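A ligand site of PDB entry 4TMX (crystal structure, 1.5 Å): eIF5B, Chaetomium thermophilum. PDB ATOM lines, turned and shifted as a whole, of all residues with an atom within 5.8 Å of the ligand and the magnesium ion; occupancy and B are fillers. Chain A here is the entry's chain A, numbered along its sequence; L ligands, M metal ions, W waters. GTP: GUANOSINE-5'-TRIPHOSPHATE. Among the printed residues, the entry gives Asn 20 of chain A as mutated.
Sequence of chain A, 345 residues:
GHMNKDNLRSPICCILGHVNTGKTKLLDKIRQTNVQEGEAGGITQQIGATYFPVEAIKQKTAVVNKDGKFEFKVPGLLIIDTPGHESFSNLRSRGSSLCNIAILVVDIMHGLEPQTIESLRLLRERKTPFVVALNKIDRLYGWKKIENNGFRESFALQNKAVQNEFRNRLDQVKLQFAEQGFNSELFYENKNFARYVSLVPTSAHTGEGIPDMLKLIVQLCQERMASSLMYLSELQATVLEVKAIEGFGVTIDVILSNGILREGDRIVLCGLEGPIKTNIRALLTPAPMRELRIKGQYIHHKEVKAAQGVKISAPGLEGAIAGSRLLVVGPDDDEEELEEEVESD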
ATOM      1  N   GLY A  17      12.503   9.352  26.965  1.00  0.00           N
ATOM      2  CA  GLY A  17      13.445   8.419  27.552  1.00  0.00           C
ATOM      3  C   GLY A  17      14.866   8.788  27.179  1.00  0.00           C
ATOM      4  O   GLY A  17      15.116   9.540  26.226  1.00  0.00           O
ATOM      5  N   HIS A  18      15.797   8.179  27.907  1.00  0.00           N
ATOM      6  CA  HIS A  18      17.206   8.430  27.632  1.00  0.00           C
ATOM      7  C   HIS A  18      17.592   7.921  26.228  1.00  0.00           C
ATOM      8  O   HIS A  18      16.846   7.114  25.616  1.00  0.00           O
ATOM      9  CB  HIS A  18      18.047   7.756  28.759  1.00  0.00           C
ATOM     10  CG  HIS A  18      19.502   8.101  28.732  1.00  0.00           C
ATOM     11  ND1 HIS A  18      20.026   9.272  29.264  1.00  0.00           N
ATOM     12  CD2 HIS A  18      20.550   7.395  28.247  1.00  0.00           C
ATOM     13  CE1 HIS A  18      21.335   9.260  29.099  1.00  0.00           C
ATOM     14  NE2 HIS A  18      21.679   8.139  28.496  1.00  0.00           N
ATOM     15  N   VAL A  19      18.730   8.365  25.718  1.00  0.00           N
ATOM     16  CA  VAL A  19      19.079   7.968  24.337  1.00  0.00           C
ATOM     17  C   VAL A  19      19.186   6.443  24.200  1.00  0.00           C
ATOM     18  O   VAL A  19      19.660   5.751  25.096  1.00  0.00           O
ATOM     19  CB  VAL A  19      20.389   8.666  23.892  1.00  0.00           C
ATOM     20  CG1 VAL A  19      21.638   8.079  24.642  1.00  0.00           C
ATOM     21  CG2 VAL A  19      20.530   8.570  22.371  1.00  0.00           C
ATOM     22  N   ASN A  20      18.659   5.936  23.078  1.00  0.00           N
ATOM     23  CA  ASN A  20      18.792   4.524  22.694  1.00  0.00           C
ATOM     24  C   ASN A  20      18.138   3.534  23.654  1.00  0.00           C
ATOM     25  O   ASN A  20      18.513   2.360  23.700  1.00  0.00           O
ATOM     26  CB  ASN A  20      20.278   4.187  22.488  1.00  0.00           C
ATOM     27  CG  ASN A  20      20.816   4.797  21.194  1.00  0.00           C
ATOM     28  OD1 ASN A  20      20.066   4.987  20.248  1.00  0.00           O
ATOM     29  ND2 ASN A  20      22.088   5.169  21.173  1.00  0.00           N
ATOM     30  N   THR A  21      17.092   3.967  24.345  1.00  0.00           N
ATOM     31  CA  THR A  21      16.366   3.077  25.221  1.00  0.00           C
ATOM     32  C   THR A  21      15.283   2.258  24.498  1.00  0.00           C
ATOM     33  O   THR A  21      14.794   1.297  25.078  1.00  0.00           O
ATOM     34  CB  THR A  21      15.711   3.874  26.390  1.00  0.00           C
ATOM     35  OG1 THR A  21      15.019   5.023  25.875  1.00  0.00           O
ATOM     36  CG2 THR A  21      16.783   4.322  27.372  1.00  0.00           C
ATOM     37  N   GLY A  22      14.977   2.625  23.255  1.00  0.00           N
ATOM     38  CA  GLY A  22      14.049   1.868  22.405  1.00  0.00           C
ATOM     39  C   GLY A  22      12.730   2.557  22.086  1.00  0.00           C
ATOM     40  O   GLY A  22      11.783   1.879  21.672  1.00  0.00           O
ATOM     41  N   LYS A  23      12.635   3.884  22.291  1.00  0.00           N
ATOM     42  CA  LYS A  23      11.429   4.635  21.954  1.00  0.00           C
ATOM     43  C   LYS A  23      10.941   4.391  20.521  1.00  0.00           C
ATOM     44  O   LYS A  23       9.811   3.982  20.279  1.00  0.00           O
ATOM     45  CB  LYS A  23      11.675   6.142  22.151  1.00  0.00           C
ATOM     46  CG  LYS A  23      12.128   6.512  23.580  1.00  0.00           C
ATOM     47  CD  LYS A  23      12.383   8.022  23.645  1.00  0.00           C
ATOM     48  CE  LYS A  23      13.647   8.496  22.909  1.00  0.00           C
ATOM     49  NZ  LYS A  23      14.930   7.988  23.630  1.00  0.00           N
ATOM     50  N   THR A  24      11.825   4.644  19.548  1.00  0.00           N
ATOM     51  CA  THR A  24      11.458   4.495  18.143  1.00  0.00           C
ATOM     52  C   THR A  24      11.261   3.020  17.804  1.00  0.00           C
ATOM     53  O   THR A  24      10.333   2.673  17.069  1.00  0.00           O
ATOM     54  CB  THR A  24      12.519   5.152  17.269  1.00  0.00           C
ATOM     55  OG1 THR A  24      12.626   6.551  17.672  1.00  0.00           O
ATOM     56  CG2 THR A  24      12.131   5.068  15.775  1.00  0.00           C
ATOM     57  N   LYS A  25      12.140   2.160  18.330  1.00  0.00           N
ATOM     58  CA  LYS A  25      11.993   0.715  18.064  1.00  0.00           C
ATOM     59  C   LYS A  25      10.625   0.183  18.551  1.00  0.00           C
ATOM     60  O   LYS A  25      10.008  -0.651  17.848  1.00  0.00           O
ATOM     61  CB  LYS A  25      13.145  -0.068  18.721  1.00  0.00           C
ATOM     62  CG  LYS A  25      13.412  -1.413  18.020  1.00  0.00           C
ATOM     63  CD  LYS A  25      14.139  -1.170  16.695  1.00  0.00           C
ATOM     64  CE  LYS A  25      14.437  -2.513  16.026  1.00  0.00           C
ATOM     65  NZ  LYS A  25      15.039  -2.251  14.695  1.00  0.00           N
ATOM     66  N   LEU A  26      10.131   0.641  19.690  1.00  0.00           N
ATOM     67  CA  LEU A  26       8.802   0.242  20.151  1.00  0.00           C
ATOM     68  C   LEU A  26       7.755   0.691  19.140  1.00  0.00           C
ATOM     69  O   LEU A  26       6.880  -0.096  18.779  1.00  0.00           O
ATOM     70  CB  LEU A  26       8.496   0.850  21.522  1.00  0.00           C
ATOM     71  CG  LEU A  26       9.199   0.192  22.731  1.00  0.00           C
ATOM     72  CD1 LEU A  26       9.109   1.139  23.946  1.00  0.00           C
ATOM     73  CD2 LEU A  26       8.497  -1.133  23.094  1.00  0.00           C
ATOM     74  N   GLN A  36      13.723   3.391  12.554  1.00  0.00           N
ATOM     75  CA  GLN A  36      14.984   3.465  13.339  1.00  0.00           C
ATOM     76  C   GLN A  36      16.159   3.080  12.449  1.00  0.00           C
ATOM     77  O   GLN A  36      17.236   3.694  12.540  1.00  0.00           O
ATOM     78  CB  GLN A  36      14.901   2.542  14.581  1.00  0.00           C
ATOM     79  CG  GLN A  36      15.986   2.845  15.590  1.00  0.00           C
ATOM     80  CD  GLN A  36      17.311   2.188  15.326  1.00  0.00           C
ATOM     81  OE1 GLN A  36      17.389   1.176  14.614  1.00  0.00           O
ATOM     82  NE2 GLN A  36      18.375   2.741  15.895  1.00  0.00           N
ATOM     83  N   GLU A  39      17.457   6.015  10.410  1.00  0.00           N
ATOM     84  CA  GLU A  39      17.943   7.214  11.076  1.00  0.00           C
ATOM     85  C   GLU A  39      19.431   7.367  11.010  1.00  0.00           C
ATOM     86  O   GLU A  39      20.171   6.413  11.277  1.00  0.00           O
ATOM     87  CB  GLU A  39      17.530   7.199  12.534  1.00  0.00           C
ATOM     88  CG  GLU A  39      16.059   7.525  12.750  1.00  0.00           C
ATOM     89  CD  GLU A  39      15.652   7.417  14.190  1.00  0.00           C
ATOM     90  OE1 GLU A  39      16.323   6.668  14.951  1.00  0.00           O
ATOM     91  OE2 GLU A  39      14.666   8.078  14.613  1.00  0.00           O
ATOM     92  N   GLY A  42      21.416   6.141  13.938  1.00  0.00           N
ATOM     93  CA  GLY A  42      20.430   5.411  14.732  1.00  0.00           C
ATOM     94  C   GLY A  42      19.824   6.270  15.827  1.00  0.00           C
ATOM     95  O   GLY A  42      19.333   5.724  16.832  1.00  0.00           O
ATOM     96  N   ILE A  43      19.833   7.586  15.679  1.00  0.00           N
ATOM     97  CA  ILE A  43      19.229   8.437  16.710  1.00  0.00           C
ATOM     98  C   ILE A  43      18.160   9.316  16.124  1.00  0.00           C
ATOM     99  O   ILE A  43      18.239   9.787  14.984  1.00  0.00           O
ATOM    100  CB  ILE A  43      20.264   9.309  17.463  1.00  0.00           C
ATOM    101  CG1 ILE A  43      21.058  10.135  16.501  1.00  0.00           C
ATOM    102  CG2 ILE A  43      21.227   8.449  18.354  1.00  0.00           C
ATOM    103  CD1 ILE A  43      21.805  11.338  17.221  1.00  0.00           C
ATOM    104  N   THR A  44      17.116   9.511  16.917  1.00  0.00           N
ATOM    105  CA  THR A  44      16.037  10.431  16.536  1.00  0.00           C
ATOM    106  C   THR A  44      16.478  11.882  16.743  1.00  0.00           C
ATOM    107  O   THR A  44      17.093  12.211  17.771  1.00  0.00           O
ATOM    108  CB  THR A  44      14.803  10.139  17.370  1.00  0.00           C
ATOM    109  OG1 THR A  44      14.389   8.778  17.127  1.00  0.00           O
ATOM    110  CG2 THR A  44      13.664  11.117  17.025  1.00  0.00           C
ATOM    111  N   ASP A  81       6.876  10.881  19.027  1.00  0.00           N
ATOM    112  CA  ASP A  81       8.189  10.315  19.320  1.00  0.00           C
ATOM    113  C   ASP A  81       9.170  11.491  19.490  1.00  0.00           C
ATOM    114  O   ASP A  81       9.045  12.513  18.813  1.00  0.00           O
ATOM    115  CB  ASP A  81       8.605   9.389  18.163  1.00  0.00           C
ATOM    116  CG  ASP A  81       9.827   8.531  18.479  1.00  0.00           C
ATOM    117  OD1 ASP A  81      10.265   8.517  19.645  1.00  0.00           O
ATOM    118  OD2 ASP A  81      10.315   7.892  17.485  1.00  0.00           O
ATOM    119  N   THR A  82      10.108  11.379  20.426  1.00  0.00           N
ATOM    120  CA  THR A  82      11.052  12.475  20.692  1.00  0.00           C
ATOM    121  C   THR A  82      12.460  11.947  20.756  1.00  0.00           C
ATOM    122  O   THR A  82      12.671  10.790  21.088  1.00  0.00           O
ATOM    123  CB  THR A  82      10.772  13.194  22.064  1.00  0.00           C
ATOM    124  OG1 THR A  82      10.859  12.244  23.139  1.00  0.00           O
ATOM    125  CG2 THR A  82       9.386  13.820  22.060  1.00  0.00           C
ATOM    126  N   PRO A  83      13.445  12.837  20.542  1.00  0.00           N
ATOM    127  CA  PRO A  83      14.843  12.414  20.698  1.00  0.00           C
ATOM    128  C   PRO A  83      15.225  12.164  22.147  1.00  0.00           C
ATOM    129  O   PRO A  83      14.773  12.900  23.027  1.00  0.00           O
ATOM    130  CB  PRO A  83      15.652  13.635  20.219  1.00  0.00           C
ATOM    131  CG  PRO A  83      14.681  14.406  19.348  1.00  0.00           C
ATOM    132  CD  PRO A  83      13.306  14.200  19.989  1.00  0.00           C
ATOM    133  N   GLY A  84      16.071  11.184  22.381  1.00  0.00           N
ATOM    134  CA  GLY A  84      16.707  11.020  23.683  1.00  0.00           C
ATOM    135  C   GLY A  84      18.082  11.662  23.797  1.00  0.00           C
ATOM    136  O   GLY A  84      18.554  11.890  24.905  1.00  0.00           O
ATOM    137  N   HIS A  85      18.724  11.943  22.674  1.00  0.00           N
ATOM    138  CA  HIS A  85      20.086  12.486  22.732  1.00  0.00           C
ATOM    139  C   HIS A  85      20.092  13.792  23.496  1.00  0.00           C
ATOM    140  O   HIS A  85      19.163  14.604  23.387  1.00  0.00           O
ATOM    141  CB  HIS A  85      20.636  12.684  21.318  1.00  0.00           C
ATOM    142  CG  HIS A  85      22.082  13.077  21.304  1.00  0.00           C
ATOM    143  ND1 HIS A  85      22.493  14.373  21.503  1.00  0.00           N
ATOM    144  CD2 HIS A  85      23.204  12.346  21.089  1.00  0.00           C
ATOM    145  CE1 HIS A  85      23.809  14.427  21.427  1.00  0.00           C
ATOM    146  NE2 HIS A  85      24.271  13.210  21.182  1.00  0.00           N
ATOM    147  N   ASN A 135      11.931  -1.482  29.083  1.00  0.00           N
ATOM    148  CA  ASN A 135      12.254  -2.050  27.792  1.00  0.00           C
ATOM    149  C   ASN A 135      13.492  -2.956  27.773  1.00  0.00           C
ATOM    150  O   ASN A 135      14.318  -2.890  28.670  1.00  0.00           O
ATOM    151  CB  ASN A 135      12.364  -0.962  26.732  1.00  0.00           C
ATOM    152  CG  ASN A 135      12.268  -1.500  25.331  1.00  0.00           C
ATOM    153  OD1 ASN A 135      11.496  -2.406  25.052  1.00  0.00           O
ATOM    154  ND2 ASN A 135      13.063  -0.943  24.437  1.00  0.00           N
ATOM    155  N   LYS A 136      13.620  -3.739  26.710  1.00  0.00           N
ATOM    156  CA  LYS A 136      14.751  -4.644  26.497  1.00  0.00           C
ATOM    157  C   LYS A 136      14.791  -5.911  27.362  1.00  0.00           C
ATOM    158  O   LYS A 136      15.853  -6.426  27.650  1.00  0.00           O
ATOM    159  CB  LYS A 136      16.077  -3.889  26.551  1.00  0.00           C
ATOM    160  CG  LYS A 136      16.104  -2.621  25.709  1.00  0.00           C
ATOM    161  CD  LYS A 136      17.490  -2.250  25.234  1.00  0.00           C
ATOM    162  CE  LYS A 136      17.479  -0.907  24.541  1.00  0.00           C
ATOM    163  NZ  LYS A 136      18.849  -0.451  24.163  1.00  0.00           N
ATOM    164  N   ILE A 137      13.631  -6.432  27.735  1.00  0.00           N
ATOM    165  CA  ILE A 137      13.584  -7.643  28.538  1.00  0.00           C
ATOM    166  C   ILE A 137      14.215  -8.843  27.839  1.00  0.00           C
ATOM    167  O   ILE A 137      14.643  -9.776  28.496  1.00  0.00           O
ATOM    168  CB  ILE A 137      12.162  -7.999  29.029  1.00  0.00           C
ATOM    169  CG1 ILE A 137      11.229  -8.291  27.855  1.00  0.00           C
ATOM    170  CG2 ILE A 137      11.616  -6.894  29.916  1.00  0.00           C
ATOM    171  CD1 ILE A 137       9.798  -8.527  28.275  1.00  0.00           C
ATOM    172  N   ASP A 138      14.249  -8.843  26.515  1.00  0.00           N
ATOM    173  CA  ASP A 138      14.884  -9.961  25.808  1.00  0.00           C
ATOM    174  C   ASP A 138      16.399 -10.048  26.112  1.00  0.00           C
ATOM    175  O   ASP A 138      17.058 -11.069  25.793  1.00  0.00           O
ATOM    176  CB  ASP A 138      14.647  -9.802  24.319  1.00  0.00           C
ATOM    177  CG  ASP A 138      15.240  -8.488  23.788  1.00  0.00           C
ATOM    178  OD1 ASP A 138      16.352  -8.534  23.231  1.00  0.00           O
ATOM    179  OD2 ASP A 138      14.620  -7.439  24.020  1.00  0.00           O
ATOM    180  N   ARG A 139      16.967  -8.982  26.688  1.00  0.00           N
ATOM    181  CA  ARG A 139      18.351  -9.008  27.126  1.00  0.00           C
ATOM    182  C   ARG A 139      18.591  -9.700  28.481  1.00  0.00           C
ATOM    183  O   ARG A 139      19.707  -9.917  28.844  1.00  0.00           O
ATOM    184  CB  ARG A 139      18.896  -7.551  27.153  1.00  0.00           C
ATOM    185  CG  ARG A 139      18.948  -6.937  25.747  1.00  0.00           C
ATOM    186  CD  ARG A 139      19.955  -5.811  25.586  1.00  0.00           C
ATOM    187  NE  ARG A 139      21.310  -6.322  25.737  1.00  0.00           N
ATOM    188  CZ  ARG A 139      22.204  -5.881  26.617  1.00  0.00           C
ATOM    189  NH1 ARG A 139      23.397  -6.445  26.666  1.00  0.00           N
ATOM    190  NH2 ARG A 139      21.910  -4.896  27.456  1.00  0.00           N
ATOM    191  N   THR A 202       8.748  -4.624  28.547  1.00  0.00           N
ATOM    192  CA  THR A 202       8.541  -4.738  27.105  1.00  0.00           C
ATOM    193  C   THR A 202       9.820  -5.199  26.448  1.00  0.00           C
ATOM    194  O   THR A 202      10.934  -5.033  26.979  1.00  0.00           O
ATOM    195  CB  THR A 202       8.113  -3.381  26.432  1.00  0.00           C
ATOM    196  OG1 THR A 202       9.150  -2.401  26.639  1.00  0.00           O
ATOM    197  CG2 THR A 202       6.826  -2.855  27.050  1.00  0.00           C
ATOM    198  N   SER A 203       9.662  -5.729  25.236  1.00  0.00           N
ATOM    199  CA  SER A 203      10.756  -5.818  24.296  1.00  0.00           C
ATOM    200  C   SER A 203      10.269  -5.259  22.974  1.00  0.00           C
ATOM    201  O   SER A 203       9.309  -5.791  22.422  1.00  0.00           O
ATOM    202  CB  SER A 203      11.206  -7.258  24.087  1.00  0.00           C
ATOM    203  OG  SER A 203      12.117  -7.327  22.987  1.00  0.00           O
ATOM    204  N   ALA A 204      10.924  -4.234  22.461  1.00  0.00           N
ATOM    205  CA  ALA A 204      10.664  -3.785  21.102  1.00  0.00           C
ATOM    206  C   ALA A 204      11.148  -4.748  20.061  1.00  0.00           C
ATOM    207  O   ALA A 204      10.681  -4.695  18.927  1.00  0.00           O
ATOM    208  CB  ALA A 204      11.332  -2.401  20.873  1.00  0.00           C
ATOM    209  N   HIS A 205      12.097  -5.625  20.404  1.00  0.00           N
ATOM    210  CA  HIS A 205      12.567  -6.575  19.431  1.00  0.00           C
ATOM    211  C   HIS A 205      11.581  -7.731  19.252  1.00  0.00           C
ATOM    212  O   HIS A 205      11.263  -8.102  18.116  1.00  0.00           O
ATOM    213  CB  HIS A 205      13.976  -7.053  19.814  1.00  0.00           C
ATOM    214  CG  HIS A 205      15.051  -6.084  19.398  1.00  0.00           C
ATOM    215  ND1 HIS A 205      16.387  -6.422  19.354  1.00  0.00           N
ATOM    216  CD2 HIS A 205      14.972  -4.795  18.972  1.00  0.00           C
ATOM    217  CE1 HIS A 205      17.077  -5.381  18.925  1.00  0.00           C
ATOM    218  NE2 HIS A 205      16.247  -4.387  18.680  1.00  0.00           N
ATOM    219  N   THR A 206      11.052  -8.259  20.361  1.00  0.00           N
ATOM    220  CA  THR A 206      10.128  -9.411  20.246  1.00  0.00           C
ATOM    221  C   THR A 206       8.661  -9.018  20.258  1.00  0.00           C
ATOM    222  O   THR A 206       7.816  -9.837  19.920  1.00  0.00           O
ATOM    223  CB  THR A 206      10.290 -10.418  21.413  1.00  0.00           C
ATOM    224  OG1 THR A 206       9.763  -9.806  22.607  1.00  0.00           O
ATOM    225  CG2 THR A 206      11.744 -10.801  21.606  1.00  0.00           C
ATOM    226  N   ARG A 293       7.233  12.490  10.387  1.00  0.00           N
ATOM    227  CA  ARG A 293       8.577  13.016  10.153  1.00  0.00           C
ATOM    228  C   ARG A 293       9.242  12.334   8.944  1.00  0.00           C
ATOM    229  O   ARG A 293      10.365  12.684   8.577  1.00  0.00           O
ATOM    230  CB  ARG A 293       9.459  12.911  11.426  1.00  0.00           C
ATOM    231  CG  ARG A 293       9.676  11.501  11.957  1.00  0.00           C
ATOM    232  CD  ARG A 293      10.619  11.501  13.166  1.00  0.00           C
ATOM    233  NE  ARG A 293      10.679  10.351  14.050  1.00  0.00           N
ATOM    234  CZ  ARG A 293      11.742   9.552  14.211  1.00  0.00           C
ATOM    235  NH1 ARG A 293      12.922   9.729  13.559  1.00  0.00           N
ATOM    236  NH2 ARG A 293      11.673   8.554  15.060  1.00  0.00           N
HETATM  237  PG  GTP L   1      16.869   7.923  20.466  1.00  0.00           P
HETATM  238  O1G GTP L   1      18.087   8.094  19.605  1.00  0.00           O
HETATM  239  O2G GTP L   1      17.004   8.469  21.855  1.00  0.00           O
HETATM  240  O3G GTP L   1      15.608   8.344  19.797  1.00  0.00           O
HETATM  241  O3B GTP L   1      16.786   6.317  20.620  1.00  0.00           O
HETATM  242  PB  GTP L   1      15.461   5.433  20.929  1.00  0.00           P
HETATM  243  O1B GTP L   1      14.418   5.729  19.911  1.00  0.00           O
HETATM  244  O2B GTP L   1      15.121   5.537  22.380  1.00  0.00           O
HETATM  245  O3A GTP L   1      16.035   3.940  20.716  1.00  0.00           O
HETATM  246  PA  GTP L   1      16.179   3.197  19.295  1.00  0.00           P
HETATM  247  O1A GTP L   1      17.044   4.038  18.407  1.00  0.00           O
HETATM  248  O2A GTP L   1      14.830   2.770  18.805  1.00  0.00           O
HETATM  249  O5' GTP L   1      16.983   1.874  19.712  1.00  0.00           O
HETATM  250  C5' GTP L   1      18.343   2.002  20.072  1.00  0.00           C
HETATM  251  C4' GTP L   1      19.022   0.647  19.943  1.00  0.00           C
HETATM  252  O4' GTP L   1      18.464  -0.222  20.924  1.00  0.00           O
HETATM  253  C3' GTP L   1      18.762   0.005  18.593  1.00  0.00           C
HETATM  254  O3' GTP L   1      19.915  -0.739  18.214  1.00  0.00           O
HETATM  255  C2' GTP L   1      17.625  -0.947  18.868  1.00  0.00           C
HETATM  256  O2' GTP L   1      17.608  -2.047  17.955  1.00  0.00           O
HETATM  257  C1' GTP L   1      17.949  -1.383  20.290  1.00  0.00           C
HETATM  258  N9  GTP L   1      16.733  -1.808  20.978  1.00  0.00           N
HETATM  259  C8  GTP L   1      15.610  -1.095  21.132  1.00  0.00           C
HETATM  260  N7  GTP L   1      14.689  -1.784  21.831  1.00  0.00           N
HETATM  261  C5  GTP L   1      15.218  -2.970  22.114  1.00  0.00           C
HETATM  262  C6  GTP L   1      14.776  -4.186  22.817  1.00  0.00           C
HETATM  263  O6  GTP L   1      13.646  -4.241  23.305  1.00  0.00           O
HETATM  264  N1  GTP L   1      15.637  -5.193  22.898  1.00  0.00           N
HETATM  265  C2  GTP L   1      16.870  -5.144  22.369  1.00  0.00           C
HETATM  266  N2  GTP L   1      17.684  -6.213  22.491  1.00  0.00           N
HETATM  267  N3  GTP L   1      17.343  -4.076  21.699  1.00  0.00           N
HETATM  268  C4  GTP L   1      16.572  -2.980  21.559  1.00  0.00           C
HETATM  269 MG    MG M   1      14.253   7.369  18.637  1.00  0.00          MG
HETATM  270  O   HOH W   1      21.557  -1.974  20.635  1.00  0.00           O
HETATM  271  O   HOH W   2      15.693   6.265  17.460  1.00  0.00           O
HETATM  272  O   HOH W   3      21.085   1.715  16.032  1.00  0.00           O
HETATM  273  O   HOH W   4      19.867  -3.658  17.575  1.00  0.00           O
HETATM  274  O   HOH W   5      12.812   8.471  19.736  1.00  0.00           O
HETATM  275  O   HOH W   6      19.924  -2.754  22.754  1.00  0.00           O
HETATM  276  O   HOH W   7      20.292  -6.513  21.072  1.00  0.00           O
HETATM  277  O   HOH W   8      18.066  10.946  20.065  1.00  0.00           O
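OG1 of Thr 24 lies close to OD2 of Asp 81 (2.7 Å).
OG1 of Thr 44 lies close to NH2 of Arg 293 (3.4 Å).
The side-chain hydroxyl of Ser 203 is in hydrogen-bond range of the side-chain carboxylate of Asp 138, 2.7 Å away.
The backbone carbonyl oxygen (O) of His 18 is in hydrogen-bond range of the side-chain amino group (NZ) of Lys 23 (2.9 Å).
The side-chain hydroxyl of Ser 203 sits at hydrogen-bond distance from the backbone NH of His 205, at 3.1 Å.
The side-chain amide nitrogen of Gln 36 sits at hydrogen-bond distance from the backbone carbonyl oxygen of Gly 42 (3.3 Å).
The side-chain hydroxyl (OG1) of Thr 21 sits at hydrogen-bond distance from the backbone carbonyl oxygen (O) of His 18 (2.8 Å).
The backbone carbonyl oxygen of Thr 202 sits at hydrogen-bond distance from the backbone NH of Lys 136 (3.0 Å).
The magnesium ion is bound by O3G of the ligand (2.0 Å), OG1 of Thr 24 (2.1 Å), OG1 of Thr 44 (2.1 Å), O1B of the ligand (2.1 Å), water W5 (2.1 Å) and water W2 (2.2 Å).
The magnesium ion has six donor atoms within binding distance.
The backbone NH (N) of Thr 24 sits close to an oxygen (O1B) of the ligand (2.8 Å).
The backbone NH (N) of Thr 44 sits at hydrogen-bond distance from an oxygen (O1G) of the ligand (3.2 Å).
N1 of the ligand is in hydrogen-bond range of OD2 of Asp 138 (2.7 Å).
O2B of the ligand sits at hydrogen-bond distance from N of Lys 23 (3.0 Å).
The side-chain amino group (NZ) of Lys 23 lies within salt-bridge range of an oxygen (O2B) of the ligand.
The backbone NH (N) of Lys 25 sits at hydrogen-bond distance from an oxygen (O2A) of the ligand (2.8 Å).
A ring nitrogen (NE2) of His 205 is in hydrogen-bond range of an oxygen (O2') of the ligand.
N of Ala 204 sits at hydrogen-bond distance from O6 of the ligand (2.8 Å).
N of Gly 84 lies within hydrogen-bond range of O2G of the ligand (2.9 Å).
The backbone NH of Gly 22 sits at hydrogen-bond distance from an oxygen (O2B) of the ligand (3.0 Å).
The backbone NH of Asn 20 is in hydrogen-bond range of an oxygen (O3B) of the ligand (3.1 Å).
NE2 of Gln 36 sits at hydrogen-bond distance from O1A of the ligand (3.1 Å).
ND2 of Asn 135 sits at hydrogen-bond distance from N7 of the ligand (3.2 Å).
N of Thr 21 sits at hydrogen-bond distance from O2B of the ligand (3.2 Å).
An oxygen (O6) of the ligand sits close to the backbone NH (N) of Lys 136, at 3.4 Å.
An oxygen (O4') of the ligand is in hydrogen-bond range of the side-chain amino group (NZ) of Lys 136 (3.3 Å).
The side-chain hydroxyl (OG) of Ser 203 sits close to an oxygen (O6) of the ligand (3.5 Å).
Along chain A the residues within 4 Å of the magnesium ion span positions 24 to 44.
Water W2 bridges OE1 of Glu 39 and O1A of the ligand.
Water W5 bridges the side-chain carboxylate (OD1) of Asp 81 (2.5 Å) and the backbone carbonyl oxygen (O) of Thr 82 (2.7 Å).
Water W8 lies within hydrogen-bond range of O of Thr 44 (2.8 Å), N of His 85 (2.9 Å), O1G of the ligand (2.9 Å) and N of Gly 84 (3.1 Å).
Water W6 lies within hydrogen-bond range of NZ of Lys 136 (2.9 Å) and N3 of the ligand (3.1 Å).
Water W3 bridges NE2 of Gln 36 (2.9 Å) and O3' of the ligand (3.5 Å).
O1A of the ligand sits close to O of Gly 42 (3.3 Å).
Merely in contact with the ligand: His 18 (3.99 Å), Val 19 (3.3 Å), Ile 43 (3.1 Å), His 85 (3.96 Å) and Arg 139 (3.6 Å).
Of the 31 residues printed, 21 come within 4 Å of the ligand.
Along chain A the residues within 4 Å of the ligand span positions 18 to 205.
The nearest printed residue that does not touch the ligand is Thr 82 (4.03 Å).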
